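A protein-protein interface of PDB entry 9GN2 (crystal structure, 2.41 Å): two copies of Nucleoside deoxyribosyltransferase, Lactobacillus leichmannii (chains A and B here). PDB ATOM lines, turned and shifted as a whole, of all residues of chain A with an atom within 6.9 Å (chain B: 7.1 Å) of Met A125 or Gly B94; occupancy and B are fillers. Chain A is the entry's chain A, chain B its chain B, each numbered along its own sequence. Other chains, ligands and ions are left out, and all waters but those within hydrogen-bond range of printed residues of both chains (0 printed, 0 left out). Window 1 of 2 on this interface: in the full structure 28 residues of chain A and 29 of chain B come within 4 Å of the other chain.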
ATOM      1  N   TYR A  86     -11.666  15.026  18.821  1.00  0.00           N
ATOM      2  CA  TYR A  86     -12.513  14.534  19.885  1.00  0.00           C
ATOM      3  C   TYR A  86     -12.064  15.075  21.244  1.00  0.00           C
ATOM      4  O   TYR A  86     -10.941  14.805  21.674  1.00  0.00           O
ATOM      5  CB  TYR A  86     -12.360  13.017  19.803  1.00  0.00           C
ATOM      6  CG  TYR A  86     -13.491  12.284  20.483  1.00  0.00           C
ATOM      7  CD1 TYR A  86     -13.454  12.027  21.841  1.00  0.00           C
ATOM      8  CD2 TYR A  86     -14.601  11.864  19.762  1.00  0.00           C
ATOM      9  CE1 TYR A  86     -14.495  11.356  22.466  1.00  0.00           C
ATOM     10  CE2 TYR A  86     -15.654  11.221  20.379  1.00  0.00           C
ATOM     11  CZ  TYR A  86     -15.612  10.988  21.736  1.00  0.00           C
ATOM     12  OH  TYR A  86     -16.679  10.330  22.298  1.00  0.00           O
ATOM     13  N   GLU A  91     -18.056  15.931  24.365  1.00  0.00           N
ATOM     14  CA  GLU A  91     -18.281  15.109  23.189  1.00  0.00           C
ATOM     15  C   GLU A  91     -19.478  15.664  22.421  1.00  0.00           C
ATOM     16  O   GLU A  91     -20.395  16.240  23.010  1.00  0.00           O
ATOM     17  CB  GLU A  91     -18.410  13.649  23.609  1.00  0.00           C
ATOM     18  CG  GLU A  91     -17.156  13.080  24.283  1.00  0.00           C
ATOM     19  CD  GLU A  91     -17.384  11.771  25.046  1.00  0.00           C
ATOM     20  OE1 GLU A  91     -18.276  11.820  25.929  1.00  0.00           O
ATOM     21  OE2 GLU A  91     -16.737  10.705  24.760  1.00  0.00           O
ATOM     22  N   ASP A  92     -19.442  15.479  21.092  1.00  0.00           N
ATOM     23  CA  ASP A  92     -20.341  16.129  20.154  1.00  0.00           C
ATOM     24  C   ASP A  92     -21.260  15.105  19.493  1.00  0.00           C
ATOM     25  O   ASP A  92     -20.803  14.194  18.778  1.00  0.00           O
ATOM     26  CB  ASP A  92     -19.565  16.885  19.087  1.00  0.00           C
ATOM     27  CG  ASP A  92     -20.442  17.701  18.153  1.00  0.00           C
ATOM     28  OD1 ASP A  92     -21.169  18.589  18.652  1.00  0.00           O
ATOM     29  OD2 ASP A  92     -20.411  17.432  16.949  1.00  0.00           O
ATOM     30  N   VAL A  93     -22.577  15.305  19.670  1.00  0.00           N
ATOM     31  CA  VAL A  93     -23.564  14.441  19.040  1.00  0.00           C
ATOM     32  C   VAL A  93     -23.415  14.438  17.507  1.00  0.00           C
ATOM     33  O   VAL A  93     -23.620  13.409  16.874  1.00  0.00           O
ATOM     34  CB  VAL A  93     -24.998  14.813  19.475  1.00  0.00           C
ATOM     35  CG1 VAL A  93     -25.414  16.192  18.978  1.00  0.00           C
ATOM     36  CG2 VAL A  93     -26.015  13.761  19.033  1.00  0.00           C
ATOM     37  N   GLY A  96     -20.588  12.285  16.495  1.00  0.00           N
ATOM     38  CA  GLY A  96     -21.002  10.923  16.771  1.00  0.00           C
ATOM     39  C   GLY A  96     -21.714  10.325  15.560  1.00  0.00           C
ATOM     40  O   GLY A  96     -21.331   9.255  15.074  1.00  0.00           O
ATOM     41  N   LEU A  99     -19.391   9.779  12.617  1.00  0.00           N
ATOM     42  CA  LEU A  99     -18.572   8.589  12.823  1.00  0.00           C
ATOM     43  C   LEU A  99     -19.345   7.369  12.338  1.00  0.00           C
ATOM     44  O   LEU A  99     -18.813   6.547  11.602  1.00  0.00           O
ATOM     45  CB  LEU A  99     -18.130   8.414  14.276  1.00  0.00           C
ATOM     46  CG  LEU A  99     -17.292   9.553  14.873  1.00  0.00           C
ATOM     47  CD1 LEU A  99     -17.030   9.361  16.357  1.00  0.00           C
ATOM     48  CD2 LEU A  99     -15.970   9.707  14.156  1.00  0.00           C
ATOM     49  N   ILE A 122     -13.609   7.740  27.268  1.00  0.00           N
ATOM     50  CA  ILE A 122     -14.441   8.199  26.163  1.00  0.00           C
ATOM     51  C   ILE A 122     -15.677   7.320  26.074  1.00  0.00           C
ATOM     52  O   ILE A 122     -15.695   6.206  26.605  1.00  0.00           O
ATOM     53  CB  ILE A 122     -13.677   8.223  24.828  1.00  0.00           C
ATOM     54  CG1 ILE A 122     -13.239   6.843  24.394  1.00  0.00           C
ATOM     55  CG2 ILE A 122     -12.493   9.175  24.885  1.00  0.00           C
ATOM     56  CD1 ILE A 122     -12.666   6.832  22.987  1.00  0.00           C
ATOM     57  N   ASN A 123     -16.720   7.847  25.422  1.00  0.00           N
ATOM     58  CA  ASN A 123     -17.958   7.101  25.247  1.00  0.00           C
ATOM     59  C   ASN A 123     -17.685   5.739  24.607  1.00  0.00           C
ATOM     60  O   ASN A 123     -16.953   5.646  23.621  1.00  0.00           O
ATOM     61  CB  ASN A 123     -18.918   7.865  24.348  1.00  0.00           C
ATOM     62  CG  ASN A 123     -20.307   7.296  24.430  1.00  0.00           C
ATOM     63  OD1 ASN A 123     -20.568   6.201  23.916  1.00  0.00           O
ATOM     64  ND2 ASN A 123     -21.191   8.029  25.093  1.00  0.00           N
ATOM     65  N   LEU A 124     -18.314   4.695  25.148  1.00  0.00           N
ATOM     66  CA  LEU A 124     -18.170   3.343  24.636  1.00  0.00           C
ATOM     67  C   LEU A 124     -18.382   3.305  23.124  1.00  0.00           C
ATOM     68  O   LEU A 124     -17.690   2.566  22.438  1.00  0.00           O
ATOM     69  CB  LEU A 124     -19.140   2.385  25.330  1.00  0.00           C
ATOM     70  CG  LEU A 124     -19.192   0.964  24.746  1.00  0.00           C
ATOM     71  CD1 LEU A 124     -17.901   0.169  24.966  1.00  0.00           C
ATOM     72  CD2 LEU A 124     -20.363   0.177  25.271  1.00  0.00           C
ATOM     73  N   MET A 125     -19.382   4.019  22.611  1.00  0.00           N
ATOM     74  CA  MET A 125     -19.721   3.887  21.203  1.00  0.00           C
ATOM     75  C   MET A 125     -18.681   4.592  20.330  1.00  0.00           C
ATOM     76  O   MET A 125     -18.459   4.158  19.202  1.00  0.00           O
ATOM     77  CB  MET A 125     -21.111   4.440  20.880  1.00  0.00           C
ATOM     78  CG  MET A 125     -22.199   3.978  21.819  1.00  0.00           C
ATOM     79  SD  MET A 125     -22.170   2.207  22.118  1.00  0.00           S
ATOM     80  CE  MET A 125     -23.070   1.533  20.716  1.00  0.00           C
ATOM     81  N   SER A 126     -18.074   5.673  20.832  1.00  0.00           N
ATOM     82  CA  SER A 126     -16.955   6.300  20.155  1.00  0.00           C
ATOM     83  C   SER A 126     -15.764   5.342  20.068  1.00  0.00           C
ATOM     84  O   SER A 126     -15.172   5.172  19.009  1.00  0.00           O
ATOM     85  CB  SER A 126     -16.567   7.550  20.850  1.00  0.00           C
ATOM     86  OG  SER A 126     -17.636   8.467  20.831  1.00  0.00           O
ATOM     87  N   TRP A 127     -15.449   4.710  21.196  1.00  0.00           N
ATOM     88  CA  TRP A 127     -14.416   3.692  21.309  1.00  0.00           C
ATOM     89  C   TRP A 127     -14.612   2.605  20.252  1.00  0.00           C
ATOM     90  O   TRP A 127     -13.667   2.210  19.574  1.00  0.00           O
ATOM     91  CB  TRP A 127     -14.464   3.128  22.731  1.00  0.00           C
ATOM     92  CG  TRP A 127     -13.533   1.989  23.010  1.00  0.00           C
ATOM     93  CD1 TRP A 127     -12.267   2.098  23.502  1.00  0.00           C
ATOM     94  CD2 TRP A 127     -13.778   0.588  22.834  1.00  0.00           C
ATOM     95  NE1 TRP A 127     -11.702   0.867  23.646  1.00  0.00           N
ATOM     96  CE2 TRP A 127     -12.598  -0.083  23.240  1.00  0.00           C
ATOM     97  CE3 TRP A 127     -14.853  -0.169  22.367  1.00  0.00           C
ATOM     98  CZ2 TRP A 127     -12.469  -1.464  23.185  1.00  0.00           C
ATOM     99  CZ3 TRP A 127     -14.728  -1.545  22.324  1.00  0.00           C
ATOM    100  CH2 TRP A 127     -13.557  -2.182  22.728  1.00  0.00           C
ATOM    101  N   GLY A 128     -15.861   2.170  20.091  1.00  0.00           N
ATOM    102  CA  GLY A 128     -16.197   1.049  19.225  1.00  0.00           C
ATOM    103  C   GLY A 128     -16.212   1.426  17.741  1.00  0.00           C
ATOM    104  O   GLY A 128     -15.702   0.676  16.924  1.00  0.00           O
ATOM    105  N   VAL A 129     -16.800   2.569  17.372  1.00  0.00           N
ATOM    106  CA  VAL A 129     -16.814   2.934  15.958  1.00  0.00           C
ATOM    107  C   VAL A 129     -15.398   3.159  15.444  1.00  0.00           C
ATOM    108  O   VAL A 129     -15.167   3.008  14.258  1.00  0.00           O
ATOM    109  CB  VAL A 129     -17.555   4.199  15.501  1.00  0.00           C
ATOM    110  CG1 VAL A 129     -18.903   3.890  14.906  1.00  0.00           C
ATOM    111  CG2 VAL A 129     -17.505   5.318  16.521  1.00  0.00           C
ATOM    112  N   SER A 130     -14.563   3.753  16.291  1.00  0.00           N
ATOM    113  CA  SER A 130     -13.192   4.092  15.967  1.00  0.00           C
ATOM    114  C   SER A 130     -12.440   2.860  15.505  1.00  0.00           C
ATOM    115  O   SER A 130     -12.584   1.765  16.055  1.00  0.00           O
ATOM    116  CB  SER A 130     -12.491   4.657  17.165  1.00  0.00           C
ATOM    117  OG  SER A 130     -13.207   5.821  17.526  1.00  0.00           O
ATOM    118  N   VAL A 156     -13.267   3.441  28.641  1.00  0.00           N
ATOM    119  CA  VAL A 156     -14.572   3.953  28.281  1.00  0.00           C
ATOM    120  C   VAL A 156     -15.421   4.252  29.518  1.00  0.00           C
ATOM    121  O   VAL A 156     -15.062   3.897  30.628  1.00  0.00           O
ATOM    122  CB  VAL A 156     -15.256   2.902  27.405  1.00  0.00           C
ATOM    123  CG1 VAL A 156     -14.330   2.436  26.301  1.00  0.00           C
ATOM    124  CG2 VAL A 156     -15.737   1.728  28.239  1.00  0.00           C
ATOM    125  N   TYR A 157     -16.547   4.929  29.285  1.00  0.00           N
ATOM    126  CA  TYR A 157     -17.710   4.911  30.169  1.00  0.00           C
ATOM    127  C   TYR A 157     -18.980   4.477  29.357  1.00  0.00           C
ATOM    128  O   TYR A 157     -19.874   3.851  29.992  1.00  0.00           O
ATOM    129  CB  TYR A 157     -17.836   6.304  30.783  1.00  0.00           C
ATOM    130  CG  TYR A 157     -18.231   7.392  29.790  1.00  0.00           C
ATOM    131  CD1 TYR A 157     -19.570   7.596  29.464  1.00  0.00           C
ATOM    132  CD2 TYR A 157     -17.280   8.213  29.172  1.00  0.00           C
ATOM    133  CE1 TYR A 157     -19.948   8.564  28.547  1.00  0.00           C
ATOM    134  CE2 TYR A 157     -17.650   9.191  28.259  1.00  0.00           C
ATOM    135  CZ  TYR A 157     -18.994   9.370  27.957  1.00  0.00           C
ATOM    136  OH  TYR A 157     -19.437  10.308  27.056  1.00  0.00           O
ATOM    137  OXT TYR A 157     -19.065   4.753  28.115  1.00  0.00           O
ATOM    138  N   TYR B   7     -35.174  -0.510  19.369  1.00  0.00           N
ATOM    139  CA  TYR B   7     -34.013  -0.381  20.229  1.00  0.00           C
ATOM    140  C   TYR B   7     -34.241   0.890  21.030  1.00  0.00           C
ATOM    141  O   TYR B   7     -34.534   1.949  20.456  1.00  0.00           O
ATOM    142  CB  TYR B   7     -32.704  -0.338  19.420  1.00  0.00           C
ATOM    143  CG  TYR B   7     -31.411  -0.024  20.176  1.00  0.00           C
ATOM    144  CD1 TYR B   7     -31.007   1.285  20.417  1.00  0.00           C
ATOM    145  CD2 TYR B   7     -30.571  -1.037  20.639  1.00  0.00           C
ATOM    146  CE1 TYR B   7     -29.836   1.581  21.121  1.00  0.00           C
ATOM    147  CE2 TYR B   7     -29.392  -0.751  21.331  1.00  0.00           C
ATOM    148  CZ  TYR B   7     -29.008   0.563  21.568  1.00  0.00           C
ATOM    149  OH  TYR B   7     -27.869   0.858  22.306  1.00  0.00           O
ATOM    150  N   THR B  68     -20.158  -5.348  24.956  1.00  0.00           N
ATOM    151  CA  THR B  68     -21.240  -4.423  25.252  1.00  0.00           C
ATOM    152  C   THR B  68     -21.537  -3.599  23.998  1.00  0.00           C
ATOM    153  O   THR B  68     -22.686  -3.409  23.602  1.00  0.00           O
ATOM    154  CB  THR B  68     -20.861  -3.543  26.449  1.00  0.00           C
ATOM    155  OG1 THR B  68     -20.454  -4.327  27.567  1.00  0.00           O
ATOM    156  CG2 THR B  68     -22.031  -2.710  26.946  1.00  0.00           C
ATOM    157  N   TYR B  69     -20.476  -3.104  23.367  1.00  0.00           N
ATOM    158  CA  TYR B  69     -20.606  -2.342  22.134  1.00  0.00           C
ATOM    159  C   TYR B  69     -21.305  -3.213  21.103  1.00  0.00           C
ATOM    160  O   TYR B  69     -22.239  -2.749  20.464  1.00  0.00           O
ATOM    161  CB  TYR B  69     -19.248  -1.832  21.626  1.00  0.00           C
ATOM    162  CG  TYR B  69     -19.250  -1.211  20.231  1.00  0.00           C
ATOM    163  CD1 TYR B  69     -19.692   0.090  20.024  1.00  0.00           C
ATOM    164  CD2 TYR B  69     -18.774  -1.909  19.124  1.00  0.00           C
ATOM    165  CE1 TYR B  69     -19.685   0.674  18.765  1.00  0.00           C
ATOM    166  CE2 TYR B  69     -18.747  -1.335  17.862  1.00  0.00           C
ATOM    167  CZ  TYR B  69     -19.213  -0.044  17.683  1.00  0.00           C
ATOM    168  OH  TYR B  69     -19.234   0.529  16.454  1.00  0.00           O
ATOM    169  N   ASN B  70     -20.906  -4.490  21.005  1.00  0.00           N
ATOM    170  CA  ASN B  70     -21.463  -5.353  19.980  1.00  0.00           C
ATOM    171  C   ASN B  70     -22.926  -5.678  20.260  1.00  0.00           C
ATOM    172  O   ASN B  70     -23.708  -5.865  19.321  1.00  0.00           O
ATOM    173  CB  ASN B  70     -20.592  -6.583  19.732  1.00  0.00           C
ATOM    174  CG  ASN B  70     -19.324  -6.229  18.978  1.00  0.00           C
ATOM    175  OD1 ASN B  70     -19.304  -5.341  18.136  1.00  0.00           O
ATOM    176  ND2 ASN B  70     -18.216  -6.846  19.315  1.00  0.00           N
ATOM    177  N   ASN B  71     -23.289  -5.775  21.538  1.00  0.00           N
ATOM    178  CA  ASN B  71     -24.657  -6.103  21.913  1.00  0.00           C
ATOM    179  C   ASN B  71     -25.588  -4.969  21.512  1.00  0.00           C
ATOM    180  O   ASN B  71     -26.673  -5.201  20.973  1.00  0.00           O
ATOM    181  CB  ASN B  71     -24.786  -6.408  23.398  1.00  0.00           C
ATOM    182  CG  ASN B  71     -24.814  -7.888  23.624  1.00  0.00           C
ATOM    183  OD1 ASN B  71     -23.822  -8.462  24.090  1.00  0.00           O
ATOM    184  ND2 ASN B  71     -25.910  -8.509  23.214  1.00  0.00           N
ATOM    185  N   ASP B  72     -25.127  -3.736  21.753  1.00  0.00           N
ATOM    186  CA  ASP B  72     -25.902  -2.566  21.384  1.00  0.00           C
ATOM    187  C   ASP B  72     -26.125  -2.562  19.871  1.00  0.00           C
ATOM    188  O   ASP B  72     -27.264  -2.443  19.411  1.00  0.00           O
ATOM    189  CB  ASP B  72     -25.295  -1.312  21.985  1.00  0.00           C
ATOM    190  CG  ASP B  72     -25.427  -1.185  23.499  1.00  0.00           C
ATOM    191  OD1 ASP B  72     -26.077  -2.063  24.134  1.00  0.00           O
ATOM    192  OD2 ASP B  72     -24.924  -0.174  24.025  1.00  0.00           O
ATOM    193  N   LEU B  73     -25.039  -2.764  19.101  1.00  0.00           N
ATOM    194  CA  LEU B  73     -25.130  -2.745  17.650  1.00  0.00           C
ATOM    195  C   LEU B  73     -26.115  -3.816  17.221  1.00  0.00           C
ATOM    196  O   LEU B  73     -26.954  -3.576  16.343  1.00  0.00           O
ATOM    197  CB  LEU B  73     -23.801  -2.959  16.929  1.00  0.00           C
ATOM    198  CG  LEU B  73     -22.763  -1.843  17.089  1.00  0.00           C
ATOM    199  CD1 LEU B  73     -21.766  -1.923  15.940  1.00  0.00           C
ATOM    200  CD2 LEU B  73     -23.334  -0.460  17.196  1.00  0.00           C
ATOM    201  N   ILE B  76     -29.687  -2.902  17.744  1.00  0.00           N
ATOM    202  CA  ILE B  76     -30.219  -2.017  16.720  1.00  0.00           C
ATOM    203  C   ILE B  76     -30.549  -2.808  15.457  1.00  0.00           C
ATOM    204  O   ILE B  76     -31.647  -2.692  14.896  1.00  0.00           O
ATOM    205  CB  ILE B  76     -29.281  -0.843  16.430  1.00  0.00           C
ATOM    206  CG1 ILE B  76     -29.093  -0.016  17.666  1.00  0.00           C
ATOM    207  CG2 ILE B  76     -29.820  -0.034  15.252  1.00  0.00           C
ATOM    208  CD1 ILE B  76     -28.001   1.029  17.576  1.00  0.00           C
ATOM    209  N   MET B  82     -35.487   2.246  15.258  1.00  0.00           N
ATOM    210  CA  MET B  82     -34.526   2.930  16.099  1.00  0.00           C
ATOM    211  C   MET B  82     -35.230   4.088  16.771  1.00  0.00           C
ATOM    212  O   MET B  82     -35.708   4.980  16.072  1.00  0.00           O
ATOM    213  CB  MET B  82     -33.362   3.528  15.303  1.00  0.00           C
ATOM    214  CG  MET B  82     -32.367   4.296  16.142  1.00  0.00           C
ATOM    215  SD  MET B  82     -31.525   3.219  17.310  1.00  0.00           S
ATOM    216  CE  MET B  82     -30.889   4.487  18.410  1.00  0.00           C
ATOM    217  N   GLU B  91     -26.944  16.691  24.724  1.00  0.00           N
ATOM    218  CA  GLU B  91     -26.854  15.833  23.549  1.00  0.00           C
ATOM    219  C   GLU B  91     -25.719  14.817  23.713  1.00  0.00           C
ATOM    220  O   GLU B  91     -24.689  15.154  24.275  1.00  0.00           O
ATOM    221  CB  GLU B  91     -26.738  16.708  22.310  1.00  0.00           C
ATOM    222  CG  GLU B  91     -28.030  17.456  21.984  1.00  0.00           C
ATOM    223  CD  GLU B  91     -27.839  18.440  20.840  1.00  0.00           C
ATOM    224  OE1 GLU B  91     -27.011  19.350  21.045  1.00  0.00           O
ATOM    225  OE2 GLU B  91     -28.476  18.325  19.771  1.00  0.00           O
ATOM    226  N   ASP B  92     -25.948  13.581  23.240  1.00  0.00           N
ATOM    227  CA  ASP B  92     -25.126  12.426  23.563  1.00  0.00           C
ATOM    228  C   ASP B  92     -24.385  11.912  22.320  1.00  0.00           C
ATOM    229  O   ASP B  92     -25.009  11.462  21.359  1.00  0.00           O
ATOM    230  CB  ASP B  92     -25.950  11.311  24.197  1.00  0.00           C
ATOM    231  CG  ASP B  92     -25.099  10.155  24.710  1.00  0.00           C
ATOM    232  OD1 ASP B  92     -24.200  10.407  25.547  1.00  0.00           O
ATOM    233  OD2 ASP B  92     -25.285   9.024  24.240  1.00  0.00           O
ATOM    234  N   VAL B  93     -23.044  11.942  22.361  1.00  0.00           N
ATOM    235  CA  VAL B  93     -22.211  11.408  21.291  1.00  0.00           C
ATOM    236  C   VAL B  93     -22.515   9.923  21.027  1.00  0.00           C
ATOM    237  O   VAL B  93     -22.507   9.499  19.874  1.00  0.00           O
ATOM    238  CB  VAL B  93     -20.710  11.620  21.547  1.00  0.00           C
ATOM    239  CG1 VAL B  93     -20.214  10.845  22.757  1.00  0.00           C
ATOM    240  CG2 VAL B  93     -19.874  11.275  20.326  1.00  0.00           C
ATOM    241  N   GLY B  94     -22.821   9.138  22.067  1.00  0.00           N
ATOM    242  CA  GLY B  94     -23.095   7.716  21.895  1.00  0.00           C
ATOM    243  C   GLY B  94     -24.375   7.505  21.100  1.00  0.00           C
ATOM    244  O   GLY B  94     -24.430   6.681  20.189  1.00  0.00           O
ATOM    245  N   LEU B  95     -25.404   8.285  21.436  1.00  0.00           N
ATOM    246  CA  LEU B  95     -26.681   8.180  20.757  1.00  0.00           C
ATOM    247  C   LEU B  95     -26.483   8.576  19.307  1.00  0.00           C
ATOM    248  O   LEU B  95     -27.071   7.965  18.423  1.00  0.00           O
ATOM    249  CB  LEU B  95     -27.750   9.051  21.413  1.00  0.00           C
ATOM    250  CG  LEU B  95     -29.130   9.014  20.745  1.00  0.00           C
ATOM    251  CD1 LEU B  95     -29.697   7.594  20.748  1.00  0.00           C
ATOM    252  CD2 LEU B  95     -30.077   9.977  21.462  1.00  0.00           C
ATOM    253  N   GLY B  96     -25.675   9.623  19.104  1.00  0.00           N
ATOM    254  CA  GLY B  96     -25.370  10.119  17.769  1.00  0.00           C
ATOM    255  C   GLY B  96     -24.849   8.982  16.889  1.00  0.00           C
ATOM    256  O   GLY B  96     -25.354   8.761  15.801  1.00  0.00           O
ATOM    257  N   MET B  97     -23.880   8.230  17.417  1.00  0.00           N
ATOM    258  CA  MET B  97     -23.281   7.108  16.719  1.00  0.00           C
ATOM    259  C   MET B  97     -24.345   6.061  16.393  1.00  0.00           C
ATOM    260  O   MET B  97     -24.423   5.596  15.244  1.00  0.00           O
ATOM    261  CB  MET B  97     -22.144   6.513  17.560  1.00  0.00           C
ATOM    262  CG  MET B  97     -21.407   5.360  16.908  1.00  0.00           C
ATOM    263  SD  MET B  97     -22.282   3.818  17.180  1.00  0.00           S
ATOM    264  CE  MET B  97     -21.721   2.791  15.817  1.00  0.00           C
ATOM    265  N   GLU B  98     -25.195   5.753  17.382  1.00  0.00           N
ATOM    266  CA  GLU B  98     -26.218   4.713  17.251  1.00  0.00           C
ATOM    267  C   GLU B  98     -27.193   5.110  16.140  1.00  0.00           C
ATOM    268  O   GLU B  98     -27.648   4.262  15.366  1.00  0.00           O
ATOM    269  CB  GLU B  98     -26.949   4.483  18.581  1.00  0.00           C
ATOM    270  CG  GLU B  98     -26.109   3.794  19.659  1.00  0.00           C
ATOM    271  CD  GLU B  98     -26.591   3.847  21.111  1.00  0.00           C
ATOM    272  OE1 GLU B  98     -25.997   3.185  21.998  1.00  0.00           O
ATOM    273  OE2 GLU B  98     -27.506   4.639  21.364  1.00  0.00           O
ATOM    274  N   LEU B  99     -27.496   6.412  16.056  1.00  0.00           N
ATOM    275  CA  LEU B  99     -28.398   6.932  15.040  1.00  0.00           C
ATOM    276  C   LEU B  99     -27.800   6.673  13.662  1.00  0.00           C
ATOM    277  O   LEU B  99     -28.474   6.188  12.754  1.00  0.00           O
ATOM    278  CB  LEU B  99     -28.673   8.421  15.239  1.00  0.00           C
ATOM    279  CG  LEU B  99     -29.378   8.804  16.545  1.00  0.00           C
ATOM    280  CD1 LEU B  99     -29.517  10.303  16.667  1.00  0.00           C
ATOM    281  CD2 LEU B  99     -30.764   8.147  16.683  1.00  0.00           C
ATOM    282  N   GLY B 100     -26.516   6.986  13.520  1.00  0.00           N
ATOM    283  CA  GLY B 100     -25.838   6.779  12.253  1.00  0.00           C
ATOM    284  C   GLY B 100     -25.800   5.301  11.875  1.00  0.00           C
ATOM    285  O   GLY B 100     -26.052   4.960  10.729  1.00  0.00           O
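Among the printed residues, merely in contact across the chains: Val A129 with Met B97 (3.2 Å), Gly A96 with Met B97 (3.3 Å), Gly A128 with Tyr B69 (3.3 Å), Val A93 with Asp B92 (3.4 Å), Asp A92 with Val B93 (3.4 Å), Glu A91 with Val B93 (3.4 Å), Asn A123 with Gly B94 (3.6 Å), Met A125 with Glu B98 (3.6 Å), Tyr A86 with Val B93 (3.6 Å), Asn A123 with Val B93 (3.6 Å), Val A93 with Glu B91 (3.6 Å), Ser A126 with Val B93 (3.6 Å), Gly A96 with Gly B96 (3.7 Å), Met A125 with Tyr B69 (3.7 Å), Gly A96 with Val B93 (3.7 Å), Leu A124 with Thr B68 (3.7 Å), Leu A124 with Tyr B69 (3.8 Å), Met A125 with Asp B72 (3.8 Å), Val A93 with Gly B96 (3.8 Å), Met A125 with Gly B94 (3.8 Å), Asn A123 with Asp B92 (3.9 Å) and Met A125 with Met B97 (3.9 Å).
Met A125 touches five residues of chain B. Printed residues of chain A within 4 Å of Gly B94: Asn A123 (3.6 Å) and Met A125 (3.8 Å). Printed residues of chain A within 4 Å of Met B97: Gly A96, Met A125 and Val A129. Of the printed residues of chain A, Glu B91 touches Val A93 (3.6 Å). Printed residues of chain B within 4 Å of Tyr A86: Val B93 (3.6 Å). Printed residues of chain B within 4 Å of Leu A124: Thr B68 and Tyr B69. Printed residues of chain A within 4 Å of Gly B96: Val A93 and Gly A96. The nearest residue of chain B that does not touch Met A125 is Leu B73 (4.1 Å). The nearest residue of chain A that does not touch Gly B94 is Ser A126 (5.4 Å). The nearest printed residue of chain B that does not touch Val A129 is Leu B73 (6.6 Å).
Glu A91 touches Val B93, and with the chains exchanged Val A93 touches Glu B91. Asp A92 touches Val B93, and with the chains exchanged Val A93 touches Asp B92. Val A93 touches Gly B96, and with the chains exchanged Gly A96 touches Val B93. Gly B96 touches its own counterpart, Gly A96. Positions printed for both chains: 91, 92, 93, 96 and 99. Of the 23 pairs that touch across the chains among the printed residues, 7 have their exchanged pair printed and touching as well.
Of the 17 printed residues of chain A, 11 touch a printed residue of chain B. Hydrophobic or aromatic side chains of chain B that line the printed part of chain A: Tyr B69, Val B93 and Met B97. Along chain B the printed residues that touch a printed residue of chain A span positions 68 to 98. Among the printed residues, no Asp or Glu carboxylate lies within 4 Å of a Lys or Arg side-chain nitrogen of the other chain.
OH of Tyr A86 is in hydrogen-bond range of OE2 of Glu A91. The backbone NH (N) of Asn A123 is in hydrogen-bond range of the side-chain carboxylate (OE2) of Glu A91. The side-chain amide nitrogen (ND2) of Asn A123 is in hydrogen-bond range of the side-chain hydroxyl (OH) of Tyr A157 (3.5 Å). The backbone NH (N) of Leu A124 sits at hydrogen-bond distance from the chain-end carboxylate (OXT) of Tyr A157. The backbone carbonyl oxygen (O) of Ser A126 is in hydrogen-bond range of the side-chain hydroxyl (OG) of Ser A130 (2.5 Å). The side-chain carboxylate of Glu B98 is in hydrogen-bond range of the side-chain hydroxyl of Tyr B7 (3.0 Å).
The side-chain hydroxyl (OH) of Tyr B69 is in hydrogen-bond range of the backbone NH (N) of Val A129, 3.3 Å away.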
